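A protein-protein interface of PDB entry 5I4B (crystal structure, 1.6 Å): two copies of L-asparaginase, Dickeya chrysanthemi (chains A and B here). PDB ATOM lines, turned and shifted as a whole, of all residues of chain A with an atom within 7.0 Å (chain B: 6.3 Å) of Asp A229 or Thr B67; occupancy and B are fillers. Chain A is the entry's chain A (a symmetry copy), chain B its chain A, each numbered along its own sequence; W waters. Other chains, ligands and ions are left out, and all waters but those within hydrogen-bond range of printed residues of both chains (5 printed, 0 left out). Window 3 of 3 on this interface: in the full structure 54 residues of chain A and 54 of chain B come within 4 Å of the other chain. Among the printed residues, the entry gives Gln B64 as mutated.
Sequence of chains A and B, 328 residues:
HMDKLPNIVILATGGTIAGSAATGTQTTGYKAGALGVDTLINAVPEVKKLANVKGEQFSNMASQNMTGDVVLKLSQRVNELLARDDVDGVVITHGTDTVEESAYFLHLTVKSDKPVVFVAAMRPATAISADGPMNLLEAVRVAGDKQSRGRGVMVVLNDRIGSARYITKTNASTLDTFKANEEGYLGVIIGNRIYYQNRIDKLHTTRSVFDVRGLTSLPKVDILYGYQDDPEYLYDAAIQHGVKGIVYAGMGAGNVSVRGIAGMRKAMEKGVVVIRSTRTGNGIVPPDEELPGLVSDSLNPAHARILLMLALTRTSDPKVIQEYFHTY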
ATOM      1  N   TYR A 227      33.418 -15.106 -28.599  1.00  0.00           N
ATOM      2  CA  TYR A 227      32.193 -14.307 -28.316  1.00  0.00           C
ATOM      3  C   TYR A 227      31.907 -14.372 -26.835  1.00  0.00           C
ATOM      4  O   TYR A 227      32.425 -15.242 -26.136  1.00  0.00           O
ATOM      5  CB  TYR A 227      30.993 -14.843 -29.159  1.00  0.00           C
ATOM      6  CG  TYR A 227      30.701 -16.329 -29.025  1.00  0.00           C
ATOM      7  CD1 TYR A 227      31.465 -17.290 -29.689  1.00  0.00           C
ATOM      8  CD2 TYR A 227      29.682 -16.814 -28.187  1.00  0.00           C
ATOM      9  CE1 TYR A 227      31.183 -18.616 -29.607  1.00  0.00           C
ATOM     10  CE2 TYR A 227      29.406 -18.170 -28.100  1.00  0.00           C
ATOM     11  CZ  TYR A 227      30.147 -19.062 -28.771  1.00  0.00           C
ATOM     12  OH  TYR A 227      29.925 -20.396 -28.776  1.00  0.00           O
ATOM     13  N   GLN A 228      31.014 -13.529 -26.340  1.00  0.00           N
ATOM     14  CA  GLN A 228      30.553 -13.579 -24.983  1.00  0.00           C
ATOM     15  C   GLN A 228      30.012 -14.970 -24.645  1.00  0.00           C
ATOM     16  O   GLN A 228      29.260 -15.526 -25.388  1.00  0.00           O
ATOM     17  CB  GLN A 228      29.493 -12.502 -24.704  1.00  0.00           C
ATOM     18  CG  GLN A 228      29.957 -11.071 -24.761  1.00  0.00           C
ATOM     19  CD  GLN A 228      28.898 -10.041 -24.419  1.00  0.00           C
ATOM     20  OE1 GLN A 228      27.741 -10.394 -24.247  1.00  0.00           O
ATOM     21  NE2 GLN A 228      29.279  -8.786 -24.375  1.00  0.00           N
ATOM     22  N   ASP A 229      30.396 -15.500 -23.501  1.00  0.00           N
ATOM     23  CA  ASP A 229      29.972 -16.824 -23.016  1.00  0.00           C
ATOM     24  C   ASP A 229      30.504 -18.003 -23.848  1.00  0.00           C
ATOM     25  O   ASP A 229      29.917 -19.085 -23.799  1.00  0.00           O
ATOM     26  CB  ASP A 229      28.438 -16.931 -22.964  1.00  0.00           C
ATOM     27  CG  ASP A 229      27.827 -15.844 -22.097  1.00  0.00           C
ATOM     28  OD1 ASP A 229      28.105 -15.868 -20.907  1.00  0.00           O
ATOM     29  OD2 ASP A 229      27.097 -14.954 -22.572  1.00  0.00           O
ATOM     30  N   ASP A 230      31.547 -17.828 -24.653  1.00  0.00           N
ATOM     31  CA  ASP A 230      32.051 -18.888 -25.461  1.00  0.00           C
ATOM     32  C   ASP A 230      32.482 -20.109 -24.569  1.00  0.00           C
ATOM     33  O   ASP A 230      33.025 -19.899 -23.501  1.00  0.00           O
ATOM     34  CB  ASP A 230      33.176 -18.444 -26.344  1.00  0.00           C
ATOM     35  CG  ASP A 230      34.360 -17.885 -25.577  1.00  0.00           C
ATOM     36  OD1 ASP A 230      34.340 -17.402 -24.412  1.00  0.00           O
ATOM     37  OD2 ASP A 230      35.451 -17.982 -26.180  1.00  0.00           O
ATOM     38  N   PRO A 231      32.183 -21.312 -25.021  1.00  0.00           N
ATOM     39  CA  PRO A 231      32.331 -22.441 -24.142  1.00  0.00           C
ATOM     40  C   PRO A 231      33.625 -23.222 -24.281  1.00  0.00           C
ATOM     41  O   PRO A 231      34.225 -23.365 -25.378  1.00  0.00           O
ATOM     42  CB  PRO A 231      31.188 -23.296 -24.557  1.00  0.00           C
ATOM     43  CG  PRO A 231      31.189 -23.145 -26.074  1.00  0.00           C
ATOM     44  CD  PRO A 231      31.375 -21.658 -26.207  1.00  0.00           C
ATOM     45  N   GLU A 232      34.052 -23.698 -23.137  1.00  0.00           N
ATOM     46  CA  GLU A 232      35.242 -24.569 -23.086  1.00  0.00           C
ATOM     47  C   GLU A 232      35.036 -25.863 -23.803  1.00  0.00           C
ATOM     48  O   GLU A 232      35.996 -26.402 -24.415  1.00  0.00           O
ATOM     49  CB  GLU A 232      35.579 -24.827 -21.618  1.00  0.00           C
ATOM     50  CG  GLU A 232      36.962 -25.263 -21.394  1.00  0.00           C
ATOM     51  CD  GLU A 232      37.264 -25.385 -19.873  1.00  0.00           C
ATOM     52  OE1 GLU A 232      36.771 -24.632 -19.025  1.00  0.00           O
ATOM     53  OE2 GLU A 232      38.077 -26.269 -19.639  1.00  0.00           O
ATOM     54  N   MET A 251      37.842 -12.475 -30.312  1.00  0.00           N
ATOM     55  CA  MET A 251      37.262 -11.202 -29.962  1.00  0.00           C
ATOM     56  C   MET A 251      38.357 -10.143 -30.091  1.00  0.00           C
ATOM     57  O   MET A 251      39.459 -10.292 -29.566  1.00  0.00           O
ATOM     58  CB  MET A 251      36.659 -11.200 -28.547  1.00  0.00           C
ATOM     59  CG  MET A 251      35.471 -12.156 -28.438  1.00  0.00           C
ATOM     60  SD  MET A 251      34.911 -12.409 -26.730  1.00  0.00           S
ATOM     61  CE  MET A 251      35.976 -13.754 -26.214  1.00  0.00           C
ATOM     62  N   SER A 257      38.514 -15.143 -23.579  1.00  0.00           N
ATOM     63  CA  SER A 257      37.876 -15.253 -22.259  1.00  0.00           C
ATOM     64  C   SER A 257      38.597 -16.211 -21.330  1.00  0.00           C
ATOM     65  O   SER A 257      39.347 -17.050 -21.792  1.00  0.00           O
ATOM     66  CB  SER A 257      36.444 -15.742 -22.399  1.00  0.00           C
ATOM     67  OG  SER A 257      36.277 -17.088 -22.797  1.00  0.00           O
ATOM     68  N   ARG A 259      37.288 -18.868 -20.216  1.00  0.00           N
ATOM     69  CA  ARG A 259      36.911 -20.187 -20.715  1.00  0.00           C
ATOM     70  C   ARG A 259      37.734 -20.608 -21.918  1.00  0.00           C
ATOM     71  O   ARG A 259      38.177 -21.783 -22.042  1.00  0.00           O
ATOM     72  CB  ARG A 259      35.411 -20.230 -21.070  1.00  0.00           C
ATOM     73  CG  ARG A 259      34.493 -20.034 -19.842  1.00  0.00           C
ATOM     74  CD  ARG A 259      33.021 -19.776 -20.177  1.00  0.00           C
ATOM     75  NE  ARG A 259      32.944 -18.699 -21.159  1.00  0.00           N
ATOM     76  CZ  ARG A 259      33.082 -17.411 -20.881  1.00  0.00           C
ATOM     77  NH1 ARG A 259      33.201 -16.960 -19.630  1.00  0.00           N
ATOM     78  NH2 ARG A 259      33.112 -16.518 -21.871  1.00  0.00           N
ATOM     79  N   MET B  61      35.747  -5.109 -15.769  1.00  0.00           N
ATOM     80  CA  MET B  61      36.332  -6.238 -16.451  1.00  0.00           C
ATOM     81  C   MET B  61      36.709  -5.927 -17.882  1.00  0.00           C
ATOM     82  O   MET B  61      36.188  -4.992 -18.495  1.00  0.00           O
ATOM     83  CB  MET B  61      35.323  -7.359 -16.398  1.00  0.00           C
ATOM     84  CG  MET B  61      34.149  -7.172 -17.295  1.00  0.00           C
ATOM     85  SD  MET B  61      33.068  -8.582 -17.300  1.00  0.00           S
ATOM     86  CE  MET B  61      32.076  -8.265 -15.860  1.00  0.00           C
ATOM     87  N   SER B  63      36.278  -6.702 -21.742  1.00  0.00           N
ATOM     88  CA  SER B  63      35.006  -7.112 -22.346  1.00  0.00           C
ATOM     89  C   SER B  63      35.019  -8.466 -22.949  1.00  0.00           C
ATOM     90  O   SER B  63      33.938  -9.081 -23.174  1.00  0.00           O
ATOM     91  CB  SER B  63      34.494  -6.113 -23.328  1.00  0.00           C
ATOM     92  OG  SER B  63      35.178  -6.199 -24.567  1.00  0.00           O
ATOM     93  N   GLN B  64      36.216  -9.045 -23.200  1.00  0.00           N
ATOM     94  CA  GLN B  64      36.234 -10.433 -23.637  1.00  0.00           C
ATOM     95  C   GLN B  64      35.662 -11.393 -22.559  1.00  0.00           C
ATOM     96  O   GLN B  64      35.361 -12.533 -22.855  1.00  0.00           O
ATOM     97  CB  GLN B  64      37.641 -10.907 -24.069  1.00  0.00           C
ATOM     98  CG  GLN B  64      38.701 -10.893 -22.997  1.00  0.00           C
ATOM     99  CD  GLN B  64      39.411  -9.590 -22.813  1.00  0.00           C
ATOM    100  OE1 GLN B  64      38.865  -8.509 -23.030  1.00  0.00           O
ATOM    101  NE2 GLN B  64      40.687  -9.670 -22.410  1.00  0.00           N
ATOM    102  N   ASN B  65      35.617 -10.931 -21.326  1.00  0.00           N
ATOM    103  CA  ASN B  65      35.013 -11.665 -20.229  1.00  0.00           C
ATOM    104  C   ASN B  65      33.610 -11.275 -19.845  1.00  0.00           C
ATOM    105  O   ASN B  65      33.029 -11.874 -18.964  1.00  0.00           O
ATOM    106  CB  ASN B  65      35.908 -11.588 -19.018  1.00  0.00           C
ATOM    107  CG  ASN B  65      37.087 -12.489 -19.167  1.00  0.00           C
ATOM    108  OD1 ASN B  65      36.918 -13.654 -19.479  1.00  0.00           O
ATOM    109  ND2 ASN B  65      38.228 -11.958 -19.020  1.00  0.00           N
ATOM    110  N   MET B  66      33.007 -10.341 -20.606  1.00  0.00           N
ATOM    111  CA  MET B  66      31.596  -9.989 -20.401  1.00  0.00           C
ATOM    112  C   MET B  66      30.738 -11.181 -20.730  1.00  0.00           C
ATOM    113  O   MET B  66      30.976 -11.926 -21.689  1.00  0.00           O
ATOM    114  CB  MET B  66      31.248  -8.755 -21.195  1.00  0.00           C
ATOM    115  CG  MET B  66      29.883  -8.251 -21.056  1.00  0.00           C
ATOM    116  SD  MET B  66      29.400  -7.812 -19.359  1.00  0.00           S
ATOM    117  CE  MET B  66      30.566  -6.539 -19.025  1.00  0.00           C
ATOM    118  N   THR B  67      29.740 -11.418 -19.895  1.00  0.00           N
ATOM    119  CA  THR B  67      28.863 -12.576 -20.043  1.00  0.00           C
ATOM    120  C   THR B  67      27.367 -12.100 -20.076  1.00  0.00           C
ATOM    121  O   THR B  67      27.047 -11.052 -19.543  1.00  0.00           O
ATOM    122  CB  THR B  67      28.975 -13.556 -18.850  1.00  0.00           C
ATOM    123  OG1 THR B  67      28.842 -12.857 -17.621  1.00  0.00           O
ATOM    124  CG2 THR B  67      30.320 -14.271 -18.891  1.00  0.00           C
ATOM    125  N   GLY B  68      26.511 -12.916 -20.667  1.00  0.00           N
ATOM    126  CA  GLY B  68      25.090 -12.621 -20.838  1.00  0.00           C
ATOM    127  C   GLY B  68      24.394 -12.305 -19.533  1.00  0.00           C
ATOM    128  O   GLY B  68      23.586 -11.387 -19.463  1.00  0.00           O
ATOM    129  N   ASP B  69      24.695 -13.078 -18.486  1.00  0.00           N
ATOM    130  CA  ASP B  69      24.092 -12.811 -17.193  1.00  0.00           C
ATOM    131  C   ASP B  69      24.388 -11.391 -16.702  1.00  0.00           C
ATOM    132  O   ASP B  69      23.500 -10.733 -16.107  1.00  0.00           O
ATOM    133  CB  ASP B  69      24.514 -13.888 -16.159  1.00  0.00           C
ATOM    134  CG  ASP B  69      23.895 -15.296 -16.435  1.00  0.00           C
ATOM    135  OD1 ASP B  69      22.814 -15.504 -17.069  1.00  0.00           O
ATOM    136  OD2 ASP B  69      24.552 -16.246 -15.970  1.00  0.00           O
ATOM    137  N   VAL B  70      25.602 -10.894 -16.953  1.00  0.00           N
ATOM    138  CA  VAL B  70      25.999  -9.575 -16.546  1.00  0.00           C
ATOM    139  C   VAL B  70      25.370  -8.530 -17.469  1.00  0.00           C
ATOM    140  O   VAL B  70      24.943  -7.503 -16.983  1.00  0.00           O
ATOM    141  CB  VAL B  70      27.574  -9.425 -16.454  1.00  0.00           C
ATOM    142  CG1 VAL B  70      27.987  -7.994 -16.168  1.00  0.00           C
ATOM    143  CG2 VAL B  70      28.114 -10.373 -15.367  1.00  0.00           C
ATOM    144  N   VAL B  71      25.357  -8.803 -18.761  1.00  0.00           N
ATOM    145  CA  VAL B  71      24.722  -7.879 -19.722  1.00  0.00           C
ATOM    146  C   VAL B  71      23.215  -7.697 -19.367  1.00  0.00           C
ATOM    147  O   VAL B  71      22.661  -6.603 -19.414  1.00  0.00           O
ATOM    148  CB  VAL B  71      24.888  -8.375 -21.181  1.00  0.00           C
ATOM    149  CG1 VAL B  71      24.148  -7.453 -22.118  1.00  0.00           C
ATOM    150  CG2 VAL B  71      26.359  -8.428 -21.548  1.00  0.00           C
ATOM    151  N   LEU B  72      22.580  -8.769 -18.972  1.00  0.00           N
ATOM    152  CA  LEU B  72      21.181  -8.742 -18.429  1.00  0.00           C
ATOM    153  C   LEU B  72      21.011  -7.820 -17.287  1.00  0.00           C
ATOM    154  O   LEU B  72      20.112  -6.962 -17.298  1.00  0.00           O
ATOM    155  CB  LEU B  72      20.741 -10.164 -18.038  1.00  0.00           C
ATOM    156  CG  LEU B  72      19.305 -10.358 -17.518  1.00  0.00           C
ATOM    157  CD1 LEU B  72      18.258  -9.907 -18.528  1.00  0.00           C
ATOM    158  CD2 LEU B  72      19.131 -11.836 -17.277  1.00  0.00           C
ATOM    159  N   GLU B 101      28.097  -6.566 -28.806  1.00  0.00           N
ATOM    160  CA  GLU B 101      27.179  -7.560 -28.293  1.00  0.00           C
ATOM    161  C   GLU B 101      26.360  -6.934 -27.160  1.00  0.00           C
ATOM    162  O   GLU B 101      25.100  -6.988 -27.141  1.00  0.00           O
ATOM    163  CB  GLU B 101      27.972  -8.806 -27.819  1.00  0.00           C
ATOM    164  CG  GLU B 101      28.499  -9.620 -28.960  1.00  0.00           C
ATOM    165  CD  GLU B 101      29.610 -10.615 -28.599  1.00  0.00           C
ATOM    166  OE1 GLU B 101      29.305 -11.745 -28.094  1.00  0.00           O
ATOM    167  OE2 GLU B 101      30.792 -10.274 -28.794  1.00  0.00           O
ATOM    168  N   LYS B 220      21.007 -20.629 -23.695  1.00  0.00           N
ATOM    169  CA  LYS B 220      22.375 -20.863 -24.215  1.00  0.00           C
ATOM    170  C   LYS B 220      22.398 -20.890 -25.739  1.00  0.00           C
ATOM    171  O   LYS B 220      21.668 -21.682 -26.395  1.00  0.00           O
ATOM    172  CB  LYS B 220      22.884 -22.172 -23.639  1.00  0.00           C
ATOM    173  CG  LYS B 220      24.295 -22.539 -24.016  1.00  0.00           C
ATOM    174  CD  LYS B 220      24.812 -23.726 -23.130  1.00  0.00           C
ATOM    175  CE  LYS B 220      26.271 -24.081 -23.477  1.00  0.00           C
ATOM    176  NZ  LYS B 220      27.333 -23.002 -23.706  1.00  0.00           N
ATOM    177  N   VAL B 221      23.294 -20.071 -26.314  1.00  0.00           N
ATOM    178  CA  VAL B 221      23.450 -20.048 -27.763  1.00  0.00           C
ATOM    179  C   VAL B 221      24.954 -20.071 -28.064  1.00  0.00           C
ATOM    180  O   VAL B 221      25.664 -19.256 -27.571  1.00  0.00           O
ATOM    181  CB  VAL B 221      22.767 -18.833 -28.397  1.00  0.00           C
ATOM    182  CG1 VAL B 221      23.024 -18.757 -29.888  1.00  0.00           C
ATOM    183  CG2 VAL B 221      21.260 -18.854 -28.131  1.00  0.00           C
ATOM    184  N   ASP B 222      25.375 -20.999 -28.883  1.00  0.00           N
ATOM    185  CA  ASP B 222      26.752 -21.018 -29.403  1.00  0.00           C
ATOM    186  C   ASP B 222      26.874 -20.609 -30.848  1.00  0.00           C
ATOM    187  O   ASP B 222      25.889 -20.612 -31.593  1.00  0.00           O
ATOM    188  CB  ASP B 222      27.342 -22.400 -29.131  1.00  0.00           C
ATOM    189  CG  ASP B 222      27.649 -22.572 -27.627  1.00  0.00           C
ATOM    190  OD1 ASP B 222      28.009 -21.593 -26.955  1.00  0.00           O
ATOM    191  OD2 ASP B 222      27.616 -23.706 -27.230  1.00  0.00           O
ATOM    192  N   ARG B 305      23.524 -13.916 -32.483  1.00  0.00           N
ATOM    193  CA  ARG B 305      23.441 -14.654 -31.207  1.00  0.00           C
ATOM    194  C   ARG B 305      22.620 -13.902 -30.153  1.00  0.00           C
ATOM    195  O   ARG B 305      21.813 -14.500 -29.486  1.00  0.00           O
ATOM    196  CB  ARG B 305      24.829 -15.031 -30.678  1.00  0.00           C
ATOM    197  CG  ARG B 305      24.861 -15.488 -29.233  1.00  0.00           C
ATOM    198  CD  ARG B 305      26.238 -16.040 -28.785  1.00  0.00           C
ATOM    199  NE  ARG B 305      26.123 -16.411 -27.374  1.00  0.00           N
ATOM    200  CZ  ARG B 305      26.185 -15.562 -26.404  1.00  0.00           C
ATOM    201  NH1 ARG B 305      26.428 -14.247 -26.600  1.00  0.00           N
ATOM    202  NH2 ARG B 305      25.949 -15.981 -25.176  1.00  0.00           N
ATOM    203  N   MET B 309      19.150 -15.419 -28.636  1.00  0.00           N
ATOM    204  CA  MET B 309      18.999 -15.584 -27.213  1.00  0.00           C
ATOM    205  C   MET B 309      17.740 -14.916 -26.709  1.00  0.00           C
ATOM    206  O   MET B 309      16.934 -15.568 -25.994  1.00  0.00           O
ATOM    207  CB  MET B 309      20.167 -14.991 -26.434  1.00  0.00           C
ATOM    208  CG  MET B 309      21.380 -15.861 -26.557  1.00  0.00           C
ATOM    209  SD  MET B 309      22.812 -14.928 -25.970  1.00  0.00           S
ATOM    210  CE  MET B 309      22.569 -15.053 -24.216  1.00  0.00           C
HETATM  211  O   HOH W   1      34.042 -14.447 -18.438  1.00  0.00           O
HETATM  212  O   HOH W   2      27.581 -20.305 -24.688  1.00  0.00           O
HETATM  213  O   HOH W   3      25.986 -15.658 -19.048  1.00  0.00           O
HETATM  214  O   HOH W   4      32.879 -13.792 -22.170  1.00  0.00           O
HETATM  215  O   HOH W   5      26.215 -12.737 -24.098  1.00  0.00           O
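Tyr A227 touches Glu B101. Val B221 touches Tyr A227 (O to CE2, 3.9 Å). Arg B305 touches Tyr A227 (CD to CD2, 3.6 Å). CG of Gln A228 touches O of Met B66, at 3.3 Å. Gln A228 touches Val B71 (OE1 to CG2, 3.6 Å). Thr B67 touches Asp A229. Asp B222 touches Pro A231. Met A251 touches Gln B64. O of Gln B64 touches CB of Ser A257, at 3.4 Å. OD1 of Asn B65 touches CA of Ser A257, at 3.3 Å.
Water W2 lies within hydrogen-bond range of the side-chain carboxylate of Asp B222, the backbone carbonyl oxygen of Asp A229 and the side-chain amino group of Lys B220. Water W4 lies within hydrogen-bond range of the backbone carbonyl oxygen (O) of Met B66 (2.7 Å), the guanidinium group (NH2) of Arg A259 (2.8 Å), the backbone carbonyl oxygen (O) of Gln B64 (2.9 Å) and the backbone NH (N) of Asp A229 (3.3 Å). Water W5 lies within hydrogen-bond range of OE1 of Gln A228 (2.8 Å), OD2 of Asp A229 (2.8 Å), NH1 of Arg B305 (2.9 Å) and N of Gly B68 (3.4 Å). Water W1 bridges the backbone carbonyl oxygen of Asn B65 (2.8 Å) and the guanidinium group of Arg A259 (2.9 Å). Water W3 lies within hydrogen-bond range of the side-chain carboxylate (OD1) of Asp A229, the backbone NH (N) of Asp B69 and the backbone NH (N) of Gly B68.
OD1 of Asp B222 lies within hydrogen-bond range of OH of Tyr A227, 2.9 Å away. The guanidinium group of Arg B305 is in salt-bridge range of the side-chain carboxylate of Asp A229, 3.0 Å away. The backbone NH (N) of Gly B68 is in hydrogen-bond range of the side-chain carboxylate (OD2) of Asp A229, 2.9 Å away. O of Gln A228 lies close to NH1 of Arg B305. The side-chain carboxylate of Glu B101 is in hydrogen-bond range of the backbone NH of Gln A228 (3.0 Å).
No position is printed for both chains.
Of chain B, only Thr B67 (3.2 Å), Gly B68 (2.9 Å) and Arg B305 (3.0 Å) come within 4 Å of Asp A229. Of the printed residues of chain B, Ser A257 touches Gln B64 and Asn B65. Of the printed residues of chain A, Thr B67 touches Asp A229 (3.2 Å). Printed residues of chain A within 4 Å of Gly B68: Asp A229 (2.9 Å). Of the printed residues of chain A, Asp B222 touches Tyr A227 (2.9 Å) and Pro A231 (3.4 Å). Of the printed residues of chain A, Arg B305 touches Tyr A227, Gln A228 and Asp A229. The nearest printed residue of chain B that does not touch Tyr A227 is Gln B64 (5.2 Å).
The backbone carbonyl oxygen (O) of Val B221 sits at hydrogen-bond distance from the guanidinium group (NE) of Arg B305, 2.9 Å away. OD1 of Asp A230 lies within hydrogen-bond range of OG of Ser A257 (2.5 Å). The side-chain sulfur (SD) of Met B309 sits at hydrogen-bond distance from the guanidinium group (NH2) of Arg B305 (3.4 Å). The side-chain sulfur (SD) of Met B61 lies close to the backbone NH (N) of Met B66. The side-chain amino group (NZ) of Lys B220 lies within salt-bridge range of the side-chain carboxylate (OD2) of Asp B222. The side-chain hydroxyl of Ser A257 lies close to the backbone NH of Arg A259 (3.3 Å).
Hydrophobic or aromatic side chains of chain A that line the printed part of chain B: Tyr A227, Pro A231 and Met A251. Of the 17 printed residues of chain B, 11 touch a printed residue of chain A. Hydrophobic or aromatic side chains of chain B within 4 Å of the printed part of chain A: Met B66 and Val B71. Among the printed residues, Asp or Glu carboxylates within 4 Å of a Lys or Arg side-chain nitrogen of the other chain: Asp A229 with Arg B305 (3.0 Å).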
